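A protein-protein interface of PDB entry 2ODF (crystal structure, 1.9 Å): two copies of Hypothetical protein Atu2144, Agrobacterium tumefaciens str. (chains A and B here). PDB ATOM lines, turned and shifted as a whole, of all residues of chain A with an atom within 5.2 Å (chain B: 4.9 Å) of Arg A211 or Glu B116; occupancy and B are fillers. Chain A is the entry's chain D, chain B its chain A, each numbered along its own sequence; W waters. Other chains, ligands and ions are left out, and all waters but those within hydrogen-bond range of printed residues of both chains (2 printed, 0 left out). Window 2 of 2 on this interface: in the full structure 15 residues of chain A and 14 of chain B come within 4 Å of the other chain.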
ATOM      1  N   PRO A  92     -13.385 -24.422  -6.035  1.00  0.00           N
ATOM      2  CA  PRO A  92     -13.084 -23.680  -7.264  1.00  0.00           C
ATOM      3  C   PRO A  92     -13.053 -24.619  -8.461  1.00  0.00           C
ATOM      4  O   PRO A  92     -12.801 -25.813  -8.293  1.00  0.00           O
ATOM      5  CB  PRO A  92     -11.676 -23.129  -7.002  1.00  0.00           C
ATOM      6  CG  PRO A  92     -11.047 -24.172  -6.143  1.00  0.00           C
ATOM      7  CD  PRO A  92     -12.156 -24.752  -5.283  1.00  0.00           C
ATOM      8  N   ASP A 174      -9.966 -21.226   8.568  1.00  0.00           N
ATOM      9  CA  ASP A 174      -8.737 -21.085   7.800  1.00  0.00           C
ATOM     10  C   ASP A 174      -7.738 -20.266   8.650  1.00  0.00           C
ATOM     11  O   ASP A 174      -7.753 -20.382   9.864  1.00  0.00           O
ATOM     12  CB  ASP A 174      -9.092 -20.384   6.497  1.00  0.00           C
ATOM     13  CG  ASP A 174      -8.132 -20.718   5.388  1.00  0.00           C
ATOM     14  OD1 ASP A 174      -7.134 -20.007   5.286  1.00  0.00           O
ATOM     15  OD2 ASP A 174      -8.359 -21.712   4.675  1.00  0.00           O
ATOM     16  N   PRO A 202      -8.899 -26.974   6.471  1.00  0.00           N
ATOM     17  CA  PRO A 202      -8.555 -26.256   5.236  1.00  0.00           C
ATOM     18  C   PRO A 202      -7.836 -27.119   4.185  1.00  0.00           C
ATOM     19  O   PRO A 202      -8.072 -26.934   2.991  1.00  0.00           O
ATOM     20  CB  PRO A 202      -7.650 -25.120   5.714  1.00  0.00           C
ATOM     21  CG  PRO A 202      -7.876 -25.007   7.160  1.00  0.00           C
ATOM     22  CD  PRO A 202      -8.411 -26.293   7.675  1.00  0.00           C
ATOM     23  N   THR A 207     -12.661 -24.875   3.155  1.00  0.00           N
ATOM     24  CA  THR A 207     -12.734 -23.469   3.536  1.00  0.00           C
ATOM     25  C   THR A 207     -12.756 -22.512   2.344  1.00  0.00           C
ATOM     26  O   THR A 207     -12.565 -21.318   2.502  1.00  0.00           O
ATOM     27  CB  THR A 207     -11.604 -23.094   4.514  1.00  0.00           C
ATOM     28  OG1 THR A 207     -10.331 -23.310   3.898  1.00  0.00           O
ATOM     29  CG2 THR A 207     -11.723 -23.957   5.799  1.00  0.00           C
ATOM     30  N   HIS A 208     -13.028 -23.025   1.160  1.00  0.00           N
ATOM     31  CA  HIS A 208     -13.150 -22.183  -0.050  1.00  0.00           C
ATOM     32  C   HIS A 208     -14.029 -20.941   0.131  1.00  0.00           C
ATOM     33  O   HIS A 208     -13.616 -19.828  -0.174  1.00  0.00           O
ATOM     34  CB  HIS A 208     -13.672 -23.026  -1.218  1.00  0.00           C
ATOM     35  CG  HIS A 208     -13.702 -22.291  -2.539  1.00  0.00           C
ATOM     36  ND1 HIS A 208     -12.573 -21.737  -3.108  1.00  0.00           N
ATOM     37  CD2 HIS A 208     -14.716 -22.053  -3.412  1.00  0.00           C
ATOM     38  CE1 HIS A 208     -12.888 -21.195  -4.271  1.00  0.00           C
ATOM     39  NE2 HIS A 208     -14.184 -21.372  -4.481  1.00  0.00           N
ATOM     40  N   THR A 209     -15.266 -21.117   0.601  1.00  0.00           N
ATOM     41  CA  THR A 209     -16.188 -19.996   0.753  1.00  0.00           C
ATOM     42  C   THR A 209     -15.647 -18.932   1.717  1.00  0.00           C
ATOM     43  O   THR A 209     -15.713 -17.738   1.438  1.00  0.00           O
ATOM     44  CB  THR A 209     -17.600 -20.516   1.117  1.00  0.00           C
ATOM     45  OG1 THR A 209     -18.071 -21.285  -0.003  1.00  0.00           O
ATOM     46  CG2 THR A 209     -18.556 -19.387   1.416  1.00  0.00           C
ATOM     47  N   LEU A 210     -15.017 -19.383   2.791  1.00  0.00           N
ATOM     48  CA  LEU A 210     -14.381 -18.485   3.760  1.00  0.00           C
ATOM     49  C   LEU A 210     -13.239 -17.708   3.115  1.00  0.00           C
ATOM     50  O   LEU A 210     -13.149 -16.493   3.295  1.00  0.00           O
ATOM     51  CB  LEU A 210     -13.882 -19.268   4.969  1.00  0.00           C
ATOM     52  CG  LEU A 210     -14.843 -20.135   5.785  1.00  0.00           C
ATOM     53  CD1 LEU A 210     -14.100 -20.725   7.009  1.00  0.00           C
ATOM     54  CD2 LEU A 210     -16.085 -19.321   6.180  1.00  0.00           C
ATOM     55  N   ARG A 211     -12.413 -18.420   2.342  1.00  0.00           N
ATOM     56  CA  ARG A 211     -11.301 -17.836   1.610  1.00  0.00           C
ATOM     57  C   ARG A 211     -11.767 -16.824   0.592  1.00  0.00           C
ATOM     58  O   ARG A 211     -11.111 -15.799   0.426  1.00  0.00           O
ATOM     59  CB  ARG A 211     -10.459 -18.896   0.896  1.00  0.00           C
ATOM     60  CG  ARG A 211      -9.670 -19.775   1.815  1.00  0.00           C
ATOM     61  CD  ARG A 211      -9.041 -20.945   1.089  1.00  0.00           C
ATOM     62  NE  ARG A 211      -8.150 -21.674   1.987  1.00  0.00           N
ATOM     63  CZ  ARG A 211      -7.315 -22.643   1.636  1.00  0.00           C
ATOM     64  NH1 ARG A 211      -7.195 -23.026   0.372  1.00  0.00           N
ATOM     65  NH2 ARG A 211      -6.555 -23.217   2.555  1.00  0.00           N
ATOM     66  N   LEU A 212     -12.884 -17.099  -0.086  1.00  0.00           N
ATOM     67  CA  LEU A 212     -13.455 -16.144  -1.038  1.00  0.00           C
ATOM     68  C   LEU A 212     -14.001 -14.899  -0.390  1.00  0.00           C
ATOM     69  O   LEU A 212     -13.821 -13.812  -0.928  1.00  0.00           O
ATOM     70  CB  LEU A 212     -14.601 -16.752  -1.856  1.00  0.00           C
ATOM     71  CG  LEU A 212     -14.302 -17.841  -2.892  1.00  0.00           C
ATOM     72  CD1 LEU A 212     -15.473 -18.048  -3.824  1.00  0.00           C
ATOM     73  CD2 LEU A 212     -13.061 -17.586  -3.692  1.00  0.00           C
ATOM     74  N   HIS A 213     -14.681 -15.040   0.744  1.00  0.00           N
ATOM     75  CA  HIS A 213     -15.532 -13.940   1.251  1.00  0.00           C
ATOM     76  C   HIS A 213     -15.103 -13.255   2.544  1.00  0.00           C
ATOM     77  O   HIS A 213     -15.423 -12.075   2.752  1.00  0.00           O
ATOM     78  CB  HIS A 213     -16.996 -14.427   1.361  1.00  0.00           C
ATOM     79  CG  HIS A 213     -17.554 -14.878   0.057  1.00  0.00           C
ATOM     80  ND1 HIS A 213     -17.789 -13.999  -0.980  1.00  0.00           N
ATOM     81  CD2 HIS A 213     -17.830 -16.115  -0.422  1.00  0.00           C
ATOM     82  CE1 HIS A 213     -18.241 -14.670  -2.021  1.00  0.00           C
ATOM     83  NE2 HIS A 213     -18.268 -15.956  -1.715  1.00  0.00           N
ATOM     84  N   ALA A 214     -14.449 -14.000   3.421  1.00  0.00           N
ATOM     85  CA  ALA A 214     -14.078 -13.502   4.741  1.00  0.00           C
ATOM     86  C   ALA A 214     -12.665 -12.921   4.758  1.00  0.00           C
ATOM     87  O   ALA A 214     -12.442 -11.814   5.232  1.00  0.00           O
ATOM     88  CB  ALA A 214     -14.195 -14.651   5.780  1.00  0.00           C
ATOM     89  N   LEU A 215     -11.721 -13.676   4.239  1.00  0.00           N
ATOM     90  CA  LEU A 215     -10.303 -13.387   4.469  1.00  0.00           C
ATOM     91  C   LEU A 215      -9.790 -12.100   3.833  1.00  0.00           C
ATOM     92  O   LEU A 215      -9.047 -11.349   4.508  1.00  0.00           O
ATOM     93  CB  LEU A 215      -9.434 -14.562   4.046  1.00  0.00           C
ATOM     94  CG  LEU A 215      -9.745 -15.914   4.672  1.00  0.00           C
ATOM     95  CD1 LEU A 215      -8.731 -16.939   4.162  1.00  0.00           C
ATOM     96  CD2 LEU A 215      -9.795 -15.879   6.231  1.00  0.00           C
ATOM     97  N   PRO A 216     -10.198 -11.799   2.576  1.00  0.00           N
ATOM     98  CA  PRO A 216      -9.722 -10.553   1.959  1.00  0.00           C
ATOM     99  C   PRO A 216      -9.998  -9.294   2.795  1.00  0.00           C
ATOM    100  O   PRO A 216      -9.168  -8.380   2.821  1.00  0.00           O
ATOM    101  CB  PRO A 216     -10.473 -10.511   0.611  1.00  0.00           C
ATOM    102  CG  PRO A 216     -10.751 -11.979   0.308  1.00  0.00           C
ATOM    103  CD  PRO A 216     -11.058 -12.575   1.650  1.00  0.00           C
ATOM    104  N   LEU B 114      -1.913 -17.015  -7.219  1.00  0.00           N
ATOM    105  CA  LEU B 114      -3.089 -16.260  -6.914  1.00  0.00           C
ATOM    106  C   LEU B 114      -3.990 -16.984  -5.903  1.00  0.00           C
ATOM    107  O   LEU B 114      -4.268 -18.121  -6.063  1.00  0.00           O
ATOM    108  CB  LEU B 114      -3.872 -15.997  -8.198  1.00  0.00           C
ATOM    109  CG  LEU B 114      -3.240 -15.039  -9.182  1.00  0.00           C
ATOM    110  CD1 LEU B 114      -4.186 -14.874 -10.349  1.00  0.00           C
ATOM    111  CD2 LEU B 114      -2.976 -13.706  -8.474  1.00  0.00           C
ATOM    112  N   ASP B 115      -4.479 -16.265  -4.926  1.00  0.00           N
ATOM    113  CA  ASP B 115      -5.334 -16.885  -3.926  1.00  0.00           C
ATOM    114  C   ASP B 115      -6.761 -17.056  -4.444  1.00  0.00           C
ATOM    115  O   ASP B 115      -7.122 -16.608  -5.548  1.00  0.00           O
ATOM    116  CB  ASP B 115      -5.236 -16.179  -2.543  1.00  0.00           C
ATOM    117  CG  ASP B 115      -5.782 -14.765  -2.517  1.00  0.00           C
ATOM    118  OD1 ASP B 115      -6.723 -14.394  -3.259  1.00  0.00           O
ATOM    119  OD2 ASP B 115      -5.291 -13.996  -1.663  1.00  0.00           O
ATOM    120  N   GLU B 116      -7.549 -17.782  -3.671  1.00  0.00           N
ATOM    121  CA  GLU B 116      -8.860 -18.164  -4.124  1.00  0.00           C
ATOM    122  C   GLU B 116      -9.778 -16.973  -4.360  1.00  0.00           C
ATOM    123  O   GLU B 116     -10.520 -16.970  -5.350  1.00  0.00           O
ATOM    124  CB  GLU B 116      -9.460 -19.220  -3.187  1.00  0.00           C
ATOM    125  CG  GLU B 116      -8.782 -20.575  -3.458  1.00  0.00           C
ATOM    126  CD  GLU B 116      -9.092 -21.658  -2.446  1.00  0.00           C
ATOM    127  OE1 GLU B 116     -10.248 -21.758  -1.991  1.00  0.00           O
ATOM    128  OE2 GLU B 116      -8.156 -22.417  -2.126  1.00  0.00           O
ATOM    129  N   ALA B 117      -9.714 -15.953  -3.506  1.00  0.00           N
ATOM    130  CA  ALA B 117     -10.578 -14.793  -3.716  1.00  0.00           C
ATOM    131  C   ALA B 117     -10.205 -14.084  -5.028  1.00  0.00           C
ATOM    132  O   ALA B 117     -11.077 -13.566  -5.725  1.00  0.00           O
ATOM    133  CB  ALA B 117     -10.495 -13.836  -2.564  1.00  0.00           C
ATOM    134  N   GLU B 118      -8.916 -14.055  -5.345  1.00  0.00           N
ATOM    135  CA  GLU B 118      -8.440 -13.303  -6.524  1.00  0.00           C
ATOM    136  C   GLU B 118      -8.767 -14.019  -7.853  1.00  0.00           C
ATOM    137  O   GLU B 118      -9.168 -13.371  -8.828  1.00  0.00           O
ATOM    138  CB  GLU B 118      -6.963 -12.994  -6.408  1.00  0.00           C
ATOM    139  CG  GLU B 118      -6.419 -12.179  -7.574  1.00  0.00           C
ATOM    140  CD  GLU B 118      -7.153 -10.851  -7.772  1.00  0.00           C
ATOM    141  OE1 GLU B 118      -7.600 -10.219  -6.785  1.00  0.00           O
ATOM    142  OE2 GLU B 118      -7.223 -10.394  -8.926  1.00  0.00           O
ATOM    143  N   ARG B 119      -8.603 -15.339  -7.890  1.00  0.00           N
ATOM    144  CA  ARG B 119      -9.029 -16.152  -9.015  1.00  0.00           C
ATOM    145  C   ARG B 119     -10.531 -16.025  -9.244  1.00  0.00           C
ATOM    146  O   ARG B 119     -10.977 -15.876 -10.382  1.00  0.00           O
ATOM    147  CB  ARG B 119      -8.677 -17.614  -8.809  1.00  0.00           C
ATOM    148  CG  ARG B 119      -7.139 -17.874  -8.782  1.00  0.00           C
ATOM    149  CD  ARG B 119      -6.813 -19.363  -8.841  1.00  0.00           C
ATOM    150  NE  ARG B 119      -7.036 -19.870 -10.185  1.00  0.00           N
ATOM    151  CZ  ARG B 119      -6.167 -19.765 -11.188  1.00  0.00           C
ATOM    152  NH1 ARG B 119      -4.984 -19.186 -11.022  1.00  0.00           N
ATOM    153  NH2 ARG B 119      -6.487 -20.249 -12.366  1.00  0.00           N
ATOM    154  N   PHE B 120     -11.304 -16.045  -8.171  1.00  0.00           N
ATOM    155  CA  PHE B 120     -12.733 -15.899  -8.311  1.00  0.00           C
ATOM    156  C   PHE B 120     -13.043 -14.487  -8.860  1.00  0.00           C
ATOM    157  O   PHE B 120     -13.833 -14.362  -9.758  1.00  0.00           O
ATOM    158  CB  PHE B 120     -13.511 -16.165  -7.014  1.00  0.00           C
ATOM    159  CG  PHE B 120     -14.959 -15.970  -7.193  1.00  0.00           C
ATOM    160  CD1 PHE B 120     -15.720 -16.932  -7.824  1.00  0.00           C
ATOM    161  CD2 PHE B 120     -15.536 -14.759  -6.919  1.00  0.00           C
ATOM    162  CE1 PHE B 120     -17.052 -16.721  -8.055  1.00  0.00           C
ATOM    163  CE2 PHE B 120     -16.850 -14.544  -7.166  1.00  0.00           C
ATOM    164  CZ  PHE B 120     -17.608 -15.527  -7.746  1.00  0.00           C
HETATM  165  O   HOH W   1      -8.727 -15.868  -0.500  1.00  0.00           O
HETATM  166  O   HOH W   2     -10.122 -24.317  -0.840  1.00  0.00           O
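The side-chain carboxylate (OE1) of Glu B116 is in hydrogen-bond range of a ring nitrogen (ND1) of His A208 (2.6 Å).
OE2 of Glu B116 lies within salt-bridge range of NH1 of Arg A211 (2.7 Å).
The side-chain carboxylate (OD2) of Asp A174 is in salt-bridge range of the guanidinium group (NE) of Arg A211, at 2.7 Å.
OG1 of Thr A207 sits at hydrogen-bond distance from NE of Arg A211.
The side-chain carboxylate (OD1) of Asp B115 lies close to the backbone NH (N) of Ala B117.
Arg A211 touches Ala B117.
CD2 of Leu A212 touches O of Glu B116 (3.1 Å).
Leu A212 touches Ala B117 (O to CB, 3.7 Å).
Leu A212 touches Phe B120 (CD2 to CB, 3.6 Å).
CG of Pro A216 touches CB of Ala B117 (3.4 Å).
Of the printed residues of chain B, His A208 touches Glu B116 (2.6 Å).
Of chain B, only Glu B116 and Ala B117 come within 4 Å of Arg A211.
Asp B115 touches none of the printed residues of chain A.
Printed residues of chain A within 4 Å of Glu B116: His A208 (2.6 Å), Arg A211 (2.7 Å) and Leu A212 (3.1 Å).
Of the printed residues of chain A, Ala B117 touches Arg A211, Leu A212 and Pro A216.
Of the printed residues of chain A, Phe B120 touches Leu A212 (3.6 Å).
The nearest printed residue of chain B that does not touch Arg A211 is Asp B115 (5.9 Å).
The nearest residue of chain A that does not touch Glu B116 is Pro A92 (4.8 Å).
The nearest printed residue of chain B that does not touch Leu A212 is Glu B118 (5.7 Å).
Hydrophobic or aromatic side chains of chain B within 4 Å of the printed part of chain A: Ala B117 and Phe B120.
Hydrophobic or aromatic side chains of chain A that line the printed part of chain B: His A208, Leu A212 and Pro A216.
Among the printed residues, 7 pairs touch across the chains.
No position is printed for both chains.
Of the 7 pairs that touch across the chains among the printed residues, none has its exchanged pair printed and touching as well.
Water W1 lies within hydrogen-bond range of the backbone carbonyl oxygen of Arg A211 (2.6 Å) and the backbone NH of Ala B117 (3.2 Å).
Water W2 bridges OE1 of Glu B116 (2.8 Å) and NH1 of Arg A211 (3.4 Å).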
